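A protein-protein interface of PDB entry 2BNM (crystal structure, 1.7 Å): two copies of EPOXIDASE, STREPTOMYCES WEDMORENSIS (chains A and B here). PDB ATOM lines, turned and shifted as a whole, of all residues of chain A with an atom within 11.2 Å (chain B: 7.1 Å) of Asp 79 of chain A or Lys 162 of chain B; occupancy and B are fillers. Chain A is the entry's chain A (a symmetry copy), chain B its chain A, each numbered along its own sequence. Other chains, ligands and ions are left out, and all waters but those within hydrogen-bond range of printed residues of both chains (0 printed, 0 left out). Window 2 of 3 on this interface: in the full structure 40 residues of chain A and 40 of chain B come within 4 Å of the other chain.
The indole nitrogen (NE1) of Trp 155 of chain B sits at hydrogen-bond distance from the backbone carbonyl oxygen (O) of Asp 79 of chain A.
The backbone NH of Met 153 of chain B lies within hydrogen-bond range of the backbone carbonyl oxygen of Ala 164 of chain B.
The backbone NH (N) of Lys 162 of chain B sits at hydrogen-bond distance from the backbone carbonyl oxygen (O) of Trp 155 of chain B (2.9 Å).
OD2 of Asp 79 of chain A touches CE of Lys 162 of chain B, at 3.7 Å.
CD1 of Trp 155 of chain B touches O of Asp 80 of chain A, at 3.3 Å.
Asp 80 of chain A touches Val 178 of chain B.
Gly 81 of chain A touches Val 178 of chain B (CA to CG2, 3.7 Å).
CG2 of Val 82 of chain A touches CD1 of Trp 155 of chain B (3.4 Å).
CE of Met 153 of chain B touches CG2 of Ile 84 of chain A, 3.3 Å away.
Printed residues of chain B within 4 Å of Gly 81 of chain A: Val 178 (3.7 Å).
Of the printed residues of chain A, Trp 155 of chain B touches Asp 79, Asp 80 and Val 82.
No residue of chain A comes within 4 Å of Gly 156 of chain B.
Asn 160 of chain B touches none of the printed residues of chain A.
No residue of chain A comes within 4 Å of Pro 161 of chain B.
Lys 162 of chain B touches just one residue of chain A: Asp 79 (3.7 Å).
No residue of chain A comes within 4 Å of Glu 163 of chain B.
The nearest residue of chain B that does not touch Asp 79 of chain A is Val 178 of chain B (6.5 Å).
Of the 16 printed residues of chain A, 5 touch a printed residue of chain B.
Hydrophobic or aromatic side chains of chain A that line the printed part of chain B: Val 82 and Ile 84.
Of the 15 printed residues of chain B, 4 touch a printed residue of chain A.
Printed residues of chain B that touch a printed residue of chain A: Met 153, Trp 155, Lys 162 and Val 178.
Hydrophobic or aromatic side chains of chain B within 4 Å of the printed part of chain A: Met 153, Trp 155 and Val 178.
Among the printed residues, 7 pairs touch across the chains.
No position is printed for both chains.
Of the 7 pairs that touch across the chains among the printed residues, none has its exchanged pair printed and touching as well.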
ATOM      1  N   GLY A  75     -36.117  31.466  12.254  1.00  0.00           N
ATOM      2  CA  GLY A  75     -35.704  30.380  11.362  1.00  0.00           C
ATOM      3  C   GLY A  75     -34.216  30.052  11.504  1.00  0.00           C
ATOM      4  O   GLY A  75     -33.482  30.741  12.220  1.00  0.00           O
ATOM      5  N   ASN A  76     -33.795  28.960  10.882  1.00  0.00           N
ATOM      6  CA  ASN A  76     -32.430  28.469  11.053  1.00  0.00           C
ATOM      7  C   ASN A  76     -31.651  28.507   9.745  1.00  0.00           C
ATOM      8  O   ASN A  76     -32.021  27.841   8.767  1.00  0.00           O
ATOM      9  CB  ASN A  76     -32.444  27.049  11.628  1.00  0.00           C
ATOM     10  CG  ASN A  76     -31.151  26.693  12.331  1.00  0.00           C
ATOM     11  OD1 ASN A  76     -30.076  27.019  11.849  1.00  0.00           O
ATOM     12  ND2 ASN A  76     -31.253  26.035  13.484  1.00  0.00           N
ATOM     13  N   ASP A  77     -30.568  29.285   9.730  1.00  0.00           N
ATOM     14  CA  ASP A  77     -29.750  29.457   8.546  1.00  0.00           C
ATOM     15  C   ASP A  77     -28.323  28.947   8.796  1.00  0.00           C
ATOM     16  O   ASP A  77     -27.403  29.285   8.040  1.00  0.00           O
ATOM     17  CB  ASP A  77     -29.708  30.933   8.135  1.00  0.00           C
ATOM     18  CG  ASP A  77     -29.326  31.877   9.285  1.00  0.00           C
ATOM     19  OD1 ASP A  77     -28.924  31.393  10.362  1.00  0.00           O
ATOM     20  OD2 ASP A  77     -29.436  33.131   9.165  1.00  0.00           O
ATOM     21  N   LEU A  78     -28.178  28.129   9.842  1.00  0.00           N
ATOM     22  CA  LEU A  78     -26.859  27.576  10.200  1.00  0.00           C
ATOM     23  C   LEU A  78     -26.574  26.233   9.517  1.00  0.00           C
ATOM     24  O   LEU A  78     -27.488  25.503   9.103  1.00  0.00           O
ATOM     25  CB  LEU A  78     -26.706  27.448  11.728  1.00  0.00           C
ATOM     26  CG  LEU A  78     -27.028  28.736  12.515  1.00  0.00           C
ATOM     27  CD1 LEU A  78     -26.931  28.515  14.014  1.00  0.00           C
ATOM     28  CD2 LEU A  78     -26.074  29.867  12.084  1.00  0.00           C
ATOM     29  N   ASP A  79     -25.284  25.939   9.383  1.00  0.00           N
ATOM     30  CA  ASP A  79     -24.802  24.654   8.843  1.00  0.00           C
ATOM     31  C   ASP A  79     -24.249  23.891  10.027  1.00  0.00           C
ATOM     32  O   ASP A  79     -23.116  24.136  10.449  1.00  0.00           O
ATOM     33  CB  ASP A  79     -23.710  24.947   7.816  1.00  0.00           C
ATOM     34  CG  ASP A  79     -23.075  23.680   7.236  1.00  0.00           C
ATOM     35  OD1 ASP A  79     -23.584  22.572   7.496  1.00  0.00           O
ATOM     36  OD2 ASP A  79     -22.057  23.733   6.514  1.00  0.00           O
ATOM     37  N   ASP A  80     -25.065  23.002  10.601  1.00  0.00           N
ATOM     38  CA  ASP A  80     -24.704  22.300  11.838  1.00  0.00           C
ATOM     39  C   ASP A  80     -24.181  23.272  12.890  1.00  0.00           C
ATOM     40  O   ASP A  80     -23.146  23.027  13.532  1.00  0.00           O
ATOM     41  CB  ASP A  80     -23.645  21.221  11.544  1.00  0.00           C
ATOM     42  CG  ASP A  80     -24.228  19.978  10.892  1.00  0.00           C
ATOM     43  OD1 ASP A  80     -25.396  20.003  10.408  1.00  0.00           O
ATOM     44  OD2 ASP A  80     -23.566  18.920  10.833  1.00  0.00           O
ATOM     45  N   GLY A  81     -24.896  24.383  13.070  1.00  0.00           N
ATOM     46  CA  GLY A  81     -24.603  25.304  14.173  1.00  0.00           C
ATOM     47  C   GLY A  81     -23.650  26.432  13.838  1.00  0.00           C
ATOM     48  O   GLY A  81     -23.368  27.266  14.695  1.00  0.00           O
ATOM     49  N   VAL A  82     -23.161  26.471  12.597  1.00  0.00           N
ATOM     50  CA  VAL A  82     -22.188  27.500  12.189  1.00  0.00           C
ATOM     51  C   VAL A  82     -22.605  28.230  10.932  1.00  0.00           C
ATOM     52  O   VAL A  82     -23.191  27.652  10.013  1.00  0.00           O
ATOM     53  CB  VAL A  82     -20.789  26.827  11.999  1.00  0.00           C
ATOM     54  CG1 VAL A  82     -19.781  27.746  11.282  1.00  0.00           C
ATOM     55  CG2 VAL A  82     -20.263  26.333  13.359  1.00  0.00           C
ATOM     56  N   ILE A  83     -22.275  29.513  10.873  1.00  0.00           N
ATOM     57  CA  ILE A  83     -22.309  30.224   9.614  1.00  0.00           C
ATOM     58  C   ILE A  83     -21.022  31.010   9.432  1.00  0.00           C
ATOM     59  O   ILE A  83     -20.477  31.575  10.394  1.00  0.00           O
ATOM     60  CB  ILE A  83     -23.585  31.111   9.482  1.00  0.00           C
ATOM     61  CG1 ILE A  83     -23.684  31.716   8.080  1.00  0.00           C
ATOM     62  CG2 ILE A  83     -23.700  32.175  10.593  1.00  0.00           C
ATOM     63  CD1 ILE A  83     -24.990  32.445   7.843  1.00  0.00           C
ATOM     64  N   ILE A  84     -20.526  30.991   8.203  1.00  0.00           N
ATOM     65  CA  ILE A  84     -19.257  31.636   7.909  1.00  0.00           C
ATOM     66  C   ILE A  84     -19.449  32.624   6.779  1.00  0.00           C
ATOM     67  O   ILE A  84     -20.343  32.460   5.926  1.00  0.00           O
ATOM     68  CB  ILE A  84     -18.161  30.608   7.520  1.00  0.00           C
ATOM     69  CG1 ILE A  84     -18.391  30.073   6.095  1.00  0.00           C
ATOM     70  CG2 ILE A  84     -18.051  29.450   8.545  1.00  0.00           C
ATOM     71  CD1 ILE A  84     -17.136  29.729   5.367  1.00  0.00           C
ATOM     72  N   GLN A  85     -18.619  33.663   6.780  1.00  0.00           N
ATOM     73  CA  GLN A  85     -18.617  34.642   5.715  1.00  0.00           C
ATOM     74  C   GLN A  85     -17.171  34.894   5.272  1.00  0.00           C
ATOM     75  O   GLN A  85     -16.293  35.230   6.078  1.00  0.00           O
ATOM     76  CB  GLN A  85     -19.237  35.928   6.184  1.00  0.00           C
ATOM     77  CG  GLN A  85     -19.228  37.032   5.165  1.00  0.00           C
ATOM     78  CD  GLN A  85     -19.284  38.379   5.837  1.00  0.00           C
ATOM     79  OE1 GLN A  85     -18.423  38.687   6.663  1.00  0.00           O
ATOM     80  NE2 GLN A  85     -20.316  39.150   5.546  1.00  0.00           N
ATOM     81  N   VAL A 109     -20.621  38.581   9.289  1.00  0.00           N
ATOM     82  CA  VAL A 109     -21.625  37.507   9.293  1.00  0.00           C
ATOM     83  C   VAL A 109     -22.789  37.818  10.223  1.00  0.00           C
ATOM     84  O   VAL A 109     -22.612  38.410  11.288  1.00  0.00           O
ATOM     85  CB  VAL A 109     -20.979  36.150   9.665  1.00  0.00           C
ATOM     86  CG1 VAL A 109     -20.539  36.115  11.144  1.00  0.00           C
ATOM     87  CG2 VAL A 109     -21.895  34.970   9.267  1.00  0.00           C
ATOM     88  N   ARG A 110     -23.999  37.443   9.788  1.00  0.00           N
ATOM     89  CA  ARG A 110     -25.179  37.518  10.667  1.00  0.00           C
ATOM     90  C   ARG A 110     -25.969  36.206  10.617  1.00  0.00           C
ATOM     91  O   ARG A 110     -25.783  35.362   9.723  1.00  0.00           O
ATOM     92  CB  ARG A 110     -26.112  38.690  10.251  1.00  0.00           C
ATOM     93  CG  ARG A 110     -25.494  40.100  10.411  1.00  0.00           C
ATOM     94  CD  ARG A 110     -26.496  41.239  10.419  1.00  0.00           C
ATOM     95  NE  ARG A 110     -27.240  41.376   9.163  1.00  0.00           N
ATOM     96  CZ  ARG A 110     -26.938  42.262   8.204  1.00  0.00           C
ATOM     97  NH1 ARG A 110     -25.856  43.050   8.315  1.00  0.00           N
ATOM     98  NH2 ARG A 110     -27.715  42.338   7.115  1.00  0.00           N
ATOM     99  N   THR A 111     -26.885  36.050  11.570  1.00  0.00           N
ATOM    100  CA  THR A 111     -27.719  34.830  11.594  1.00  0.00           C
ATOM    101  C   THR A 111     -29.078  35.100  12.213  1.00  0.00           C
ATOM    102  O   THR A 111     -29.182  35.783  13.227  1.00  0.00           O
ATOM    103  CB  THR A 111     -26.999  33.647  12.349  1.00  0.00           C
ATOM    104  OG1 THR A 111     -27.968  32.621  12.657  1.00  0.00           O
ATOM    105  CG2 THR A 111     -26.438  34.060  13.724  1.00  0.00           C
ATOM    106  N   LYS A 112     -30.108  34.474  11.634  1.00  0.00           N
ATOM    107  CA  LYS A 112     -31.461  34.538  12.191  1.00  0.00           C
ATOM    108  C   LYS A 112     -31.558  33.851  13.553  1.00  0.00           C
ATOM    109  O   LYS A 112     -32.507  34.093  14.296  1.00  0.00           O
ATOM    110  CB  LYS A 112     -32.392  33.806  11.220  1.00  0.00           C
ATOM    111  CG  LYS A 112     -32.628  34.527   9.905  1.00  0.00           C
ATOM    112  CD  LYS A 112     -33.299  33.462   9.022  1.00  0.00           C
ATOM    113  CE  LYS A 112     -34.308  34.014   8.113  1.00  0.00           C
ATOM    114  NZ  LYS A 112     -35.108  32.839   7.660  1.00  0.00           N
ATOM    115  N   ARG A 113     -30.600  32.979  13.862  1.00  0.00           N
ATOM    116  CA  ARG A 113     -30.533  32.342  15.203  1.00  0.00           C
ATOM    117  C   ARG A 113     -30.101  33.309  16.327  1.00  0.00           C
ATOM    118  O   ARG A 113     -30.284  33.009  17.505  1.00  0.00           O
ATOM    119  CB  ARG A 113     -29.678  31.060  15.156  1.00  0.00           C
ATOM    120  CG  ARG A 113     -30.330  29.968  14.288  1.00  0.00           C
ATOM    121  CD  ARG A 113     -31.510  29.269  14.991  1.00  0.00           C
ATOM    122  NE  ARG A 113     -30.993  28.346  16.006  1.00  0.00           N
ATOM    123  CZ  ARG A 113     -31.718  27.427  16.640  1.00  0.00           C
ATOM    124  NH1 ARG A 113     -33.019  27.303  16.378  1.00  0.00           N
ATOM    125  NH2 ARG A 113     -31.136  26.629  17.540  1.00  0.00           N
ATOM    126  N   PHE B 134     -11.046  18.976  19.588  1.00  0.00           N
ATOM    127  CA  PHE B 134     -12.391  19.526  19.725  1.00  0.00           C
ATOM    128  C   PHE B 134     -12.692  19.846  21.164  1.00  0.00           C
ATOM    129  O   PHE B 134     -12.307  19.090  22.072  1.00  0.00           O
ATOM    130  CB  PHE B 134     -13.437  18.548  19.220  1.00  0.00           C
ATOM    131  CG  PHE B 134     -13.746  18.692  17.765  1.00  0.00           C
ATOM    132  CD1 PHE B 134     -12.751  18.515  16.802  1.00  0.00           C
ATOM    133  CD2 PHE B 134     -15.039  19.004  17.354  1.00  0.00           C
ATOM    134  CE1 PHE B 134     -13.049  18.641  15.451  1.00  0.00           C
ATOM    135  CE2 PHE B 134     -15.347  19.127  16.001  1.00  0.00           C
ATOM    136  CZ  PHE B 134     -14.346  18.956  15.060  1.00  0.00           C
ATOM    137  N   HIS B 152      -7.844  27.219   9.922  1.00  0.00           N
ATOM    138  CA  HIS B 152      -8.524  25.983   9.552  1.00  0.00           C
ATOM    139  C   HIS B 152      -9.481  25.623  10.681  1.00  0.00           C
ATOM    140  O   HIS B 152      -9.078  25.190  11.784  1.00  0.00           O
ATOM    141  CB  HIS B 152      -7.491  24.858   9.278  1.00  0.00           C
ATOM    142  CG  HIS B 152      -8.103  23.586   8.774  1.00  0.00           C
ATOM    143  ND1 HIS B 152      -7.520  22.827   7.771  1.00  0.00           N
ATOM    144  CD2 HIS B 152      -9.238  22.935   9.126  1.00  0.00           C
ATOM    145  CE1 HIS B 152      -8.267  21.756   7.548  1.00  0.00           C
ATOM    146  NE2 HIS B 152      -9.314  21.797   8.351  1.00  0.00           N
ATOM    147  N   MET B 153     -10.776  25.809  10.402  1.00  0.00           N
ATOM    148  CA  MET B 153     -11.817  25.564  11.387  1.00  0.00           C
ATOM    149  C   MET B 153     -12.451  24.214  11.175  1.00  0.00           C
ATOM    150  O   MET B 153     -12.671  23.807  10.046  1.00  0.00           O
ATOM    151  CB  MET B 153     -12.870  26.658  11.273  1.00  0.00           C
ATOM    152  CG  MET B 153     -14.156  26.394  12.016  1.00  0.00           C
ATOM    153  SD  MET B 153     -15.163  27.866  11.881  1.00  0.00           S
ATOM    154  CE  MET B 153     -15.714  27.819  10.193  1.00  0.00           C
ATOM    155  N   LYS B 154     -12.745  23.539  12.268  1.00  0.00           N
ATOM    156  CA  LYS B 154     -13.521  22.300  12.239  1.00  0.00           C
ATOM    157  C   LYS B 154     -14.674  22.376  13.239  1.00  0.00           C
ATOM    158  O   LYS B 154     -14.522  22.963  14.298  1.00  0.00           O
ATOM    159  CB  LYS B 154     -12.625  21.109  12.607  1.00  0.00           C
ATOM    160  CG  LYS B 154     -11.350  20.987  11.777  1.00  0.00           C
ATOM    161  CD  LYS B 154     -10.702  19.634  12.149  1.00  0.00           C
ATOM    162  CE  LYS B 154      -9.450  19.356  11.323  1.00  0.00           C
ATOM    163  NZ  LYS B 154      -8.876  18.040  11.753  1.00  0.00           N
ATOM    164  N   TRP B 155     -15.827  21.788  12.929  1.00  0.00           N
ATOM    165  CA  TRP B 155     -16.931  21.795  13.881  1.00  0.00           C
ATOM    166  C   TRP B 155     -17.859  20.644  13.692  1.00  0.00           C
ATOM    167  O   TRP B 155     -17.776  19.947  12.679  1.00  0.00           O
ATOM    168  CB  TRP B 155     -17.734  23.098  13.793  1.00  0.00           C
ATOM    169  CG  TRP B 155     -18.624  23.291  12.585  1.00  0.00           C
ATOM    170  CD1 TRP B 155     -19.976  23.063  12.510  1.00  0.00           C
ATOM    171  CD2 TRP B 155     -18.253  23.884  11.340  1.00  0.00           C
ATOM    172  NE1 TRP B 155     -20.461  23.450  11.280  1.00  0.00           N
ATOM    173  CE2 TRP B 155     -19.428  23.960  10.536  1.00  0.00           C
ATOM    174  CE3 TRP B 155     -17.041  24.350  10.802  1.00  0.00           C
ATOM    175  CZ2 TRP B 155     -19.417  24.493   9.239  1.00  0.00           C
ATOM    176  CZ3 TRP B 155     -17.033  24.884   9.500  1.00  0.00           C
ATOM    177  CH2 TRP B 155     -18.223  24.941   8.735  1.00  0.00           C
ATOM    178  N   GLY B 156     -18.754  20.468  14.667  1.00  0.00           N
ATOM    179  CA  GLY B 156     -19.769  19.428  14.585  1.00  0.00           C
ATOM    180  C   GLY B 156     -19.248  18.129  15.162  1.00  0.00           C
ATOM    181  O   GLY B 156     -18.788  18.092  16.292  1.00  0.00           O
ATOM    182  N   ASP B 157     -19.325  17.071  14.369  1.00  0.00           N
ATOM    183  CA  ASP B 157     -18.932  15.739  14.810  1.00  0.00           C
ATOM    184  C   ASP B 157     -17.422  15.540  14.661  1.00  0.00           C
ATOM    185  O   ASP B 157     -16.900  15.507  13.542  1.00  0.00           O
ATOM    186  CB  ASP B 157     -19.723  14.709  13.988  1.00  0.00           C
ATOM    187  CG  ASP B 157     -19.319  13.278  14.267  1.00  0.00           C
ATOM    188  OD1 ASP B 157     -18.596  13.019  15.256  1.00  0.00           O
ATOM    189  OD2 ASP B 157     -19.696  12.340  13.528  1.00  0.00           O
ATOM    190  N   LYS B 158     -16.714  15.413  15.788  1.00  0.00           N
ATOM    191  CA  LYS B 158     -15.252  15.289  15.758  1.00  0.00           C
ATOM    192  C   LYS B 158     -14.766  14.144  14.856  1.00  0.00           C
ATOM    193  O   LYS B 158     -13.656  14.192  14.310  1.00  0.00           O
ATOM    194  CB  LYS B 158     -14.677  15.146  17.180  1.00  0.00           C
ATOM    195  CG  LYS B 158     -15.092  13.875  17.912  1.00  0.00           C
ATOM    196  CD  LYS B 158     -14.603  13.851  19.363  1.00  0.00           C
ATOM    197  CE  LYS B 158     -14.423  12.412  19.873  1.00  0.00           C
ATOM    198  NZ  LYS B 158     -15.566  11.488  19.559  1.00  0.00           N
ATOM    199  N   ASN B 160     -16.482  13.084  12.066  1.00  0.00           N
ATOM    200  CA  ASN B 160     -16.781  13.437  10.677  1.00  0.00           C
ATOM    201  C   ASN B 160     -17.089  14.943  10.544  1.00  0.00           C
ATOM    202  O   ASN B 160     -18.228  15.341  10.287  1.00  0.00           O
ATOM    203  CB  ASN B 160     -17.954  12.591  10.174  1.00  0.00           C
ATOM    204  CG  ASN B 160     -18.226  12.773   8.685  1.00  0.00           C
ATOM    205  OD1 ASN B 160     -19.344  12.552   8.224  1.00  0.00           O
ATOM    206  ND2 ASN B 160     -17.210  13.180   7.933  1.00  0.00           N
ATOM    207  N   PRO B 161     -16.086  15.790  10.745  1.00  0.00           N
ATOM    208  CA  PRO B 161     -16.357  17.213  10.943  1.00  0.00           C
ATOM    209  C   PRO B 161     -16.730  17.990   9.688  1.00  0.00           C
ATOM    210  O   PRO B 161     -16.337  17.635   8.565  1.00  0.00           O
ATOM    211  CB  PRO B 161     -15.018  17.746  11.475  1.00  0.00           C
ATOM    212  CG  PRO B 161     -13.989  16.852  10.885  1.00  0.00           C
ATOM    213  CD  PRO B 161     -14.641  15.492  10.807  1.00  0.00           C
ATOM    214  N   LYS B 162     -17.442  19.089   9.903  1.00  0.00           N
ATOM    215  CA  LYS B 162     -17.505  20.135   8.901  1.00  0.00           C
ATOM    216  C   LYS B 162     -16.198  20.914   9.020  1.00  0.00           C
ATOM    217  O   LYS B 162     -15.576  20.952  10.107  1.00  0.00           O
ATOM    218  CB  LYS B 162     -18.700  21.038   9.195  1.00  0.00           C
ATOM    219  CG  LYS B 162     -20.089  20.349   9.128  1.00  0.00           C
ATOM    220  CD  LYS B 162     -20.298  19.583   7.821  1.00  0.00           C
ATOM    221  CE  LYS B 162     -20.358  20.502   6.600  1.00  0.00           C
ATOM    222  NZ  LYS B 162     -20.095  19.735   5.326  1.00  0.00           N
ATOM    223  N   GLU B 163     -15.770  21.533   7.922  1.00  0.00           N
ATOM    224  CA  GLU B 163     -14.504  22.268   7.928  1.00  0.00           C
ATOM    225  C   GLU B 163     -14.589  23.517   7.079  1.00  0.00           C
ATOM    226  O   GLU B 163     -15.393  23.600   6.147  1.00  0.00           O
ATOM    227  CB  GLU B 163     -13.364  21.402   7.403  1.00  0.00           C
ATOM    228  CG  GLU B 163     -13.227  20.070   8.108  1.00  0.00           C
ATOM    229  CD  GLU B 163     -12.063  19.279   7.576  1.00  0.00           C
ATOM    230  OE1 GLU B 163     -10.928  19.510   8.053  1.00  0.00           O
ATOM    231  OE2 GLU B 163     -12.286  18.465   6.646  1.00  0.00           O
ATOM    232  N   ALA B 164     -13.744  24.489   7.390  1.00  0.00           N
ATOM    233  CA  ALA B 164     -13.625  25.678   6.556  1.00  0.00           C
ATOM    234  C   ALA B 164     -12.233  26.232   6.664  1.00  0.00           C
ATOM    235  O   ALA B 164     -11.690  26.321   7.779  1.00  0.00           O
ATOM    236  CB  ALA B 164     -14.630  26.772   6.963  1.00  0.00           C
ATOM    237  N   VAL B 178     -22.056  23.897  20.187  1.00  0.00           N
ATOM    238  CA  VAL B 178     -21.493  23.255  19.006  1.00  0.00           C
ATOM    239  C   VAL B 178     -20.011  23.002  19.216  1.00  0.00           C
ATOM    240  O   VAL B 178     -19.251  23.953  19.367  1.00  0.00           O
ATOM    241  CB  VAL B 178     -21.671  24.132  17.753  1.00  0.00           C
ATOM    242  CG1 VAL B 178     -20.991  23.506  16.529  1.00  0.00           C
ATOM    243  CG2 VAL B 178     -23.172  24.411  17.517  1.00  0.00           C
ATOM    244  N   ALA B 181     -13.042  23.361  16.786  1.00  0.00           N
ATOM    245  CA  ALA B 181     -11.587  23.485  16.962  1.00  0.00           C
ATOM    246  C   ALA B 181     -10.995  24.313  15.841  1.00  0.00           C
ATOM    247  O   ALA B 181     -11.536  24.361  14.723  1.00  0.00           O
ATOM    248  CB  ALA B 181     -10.932  22.094  16.999  1.00  0.00           C
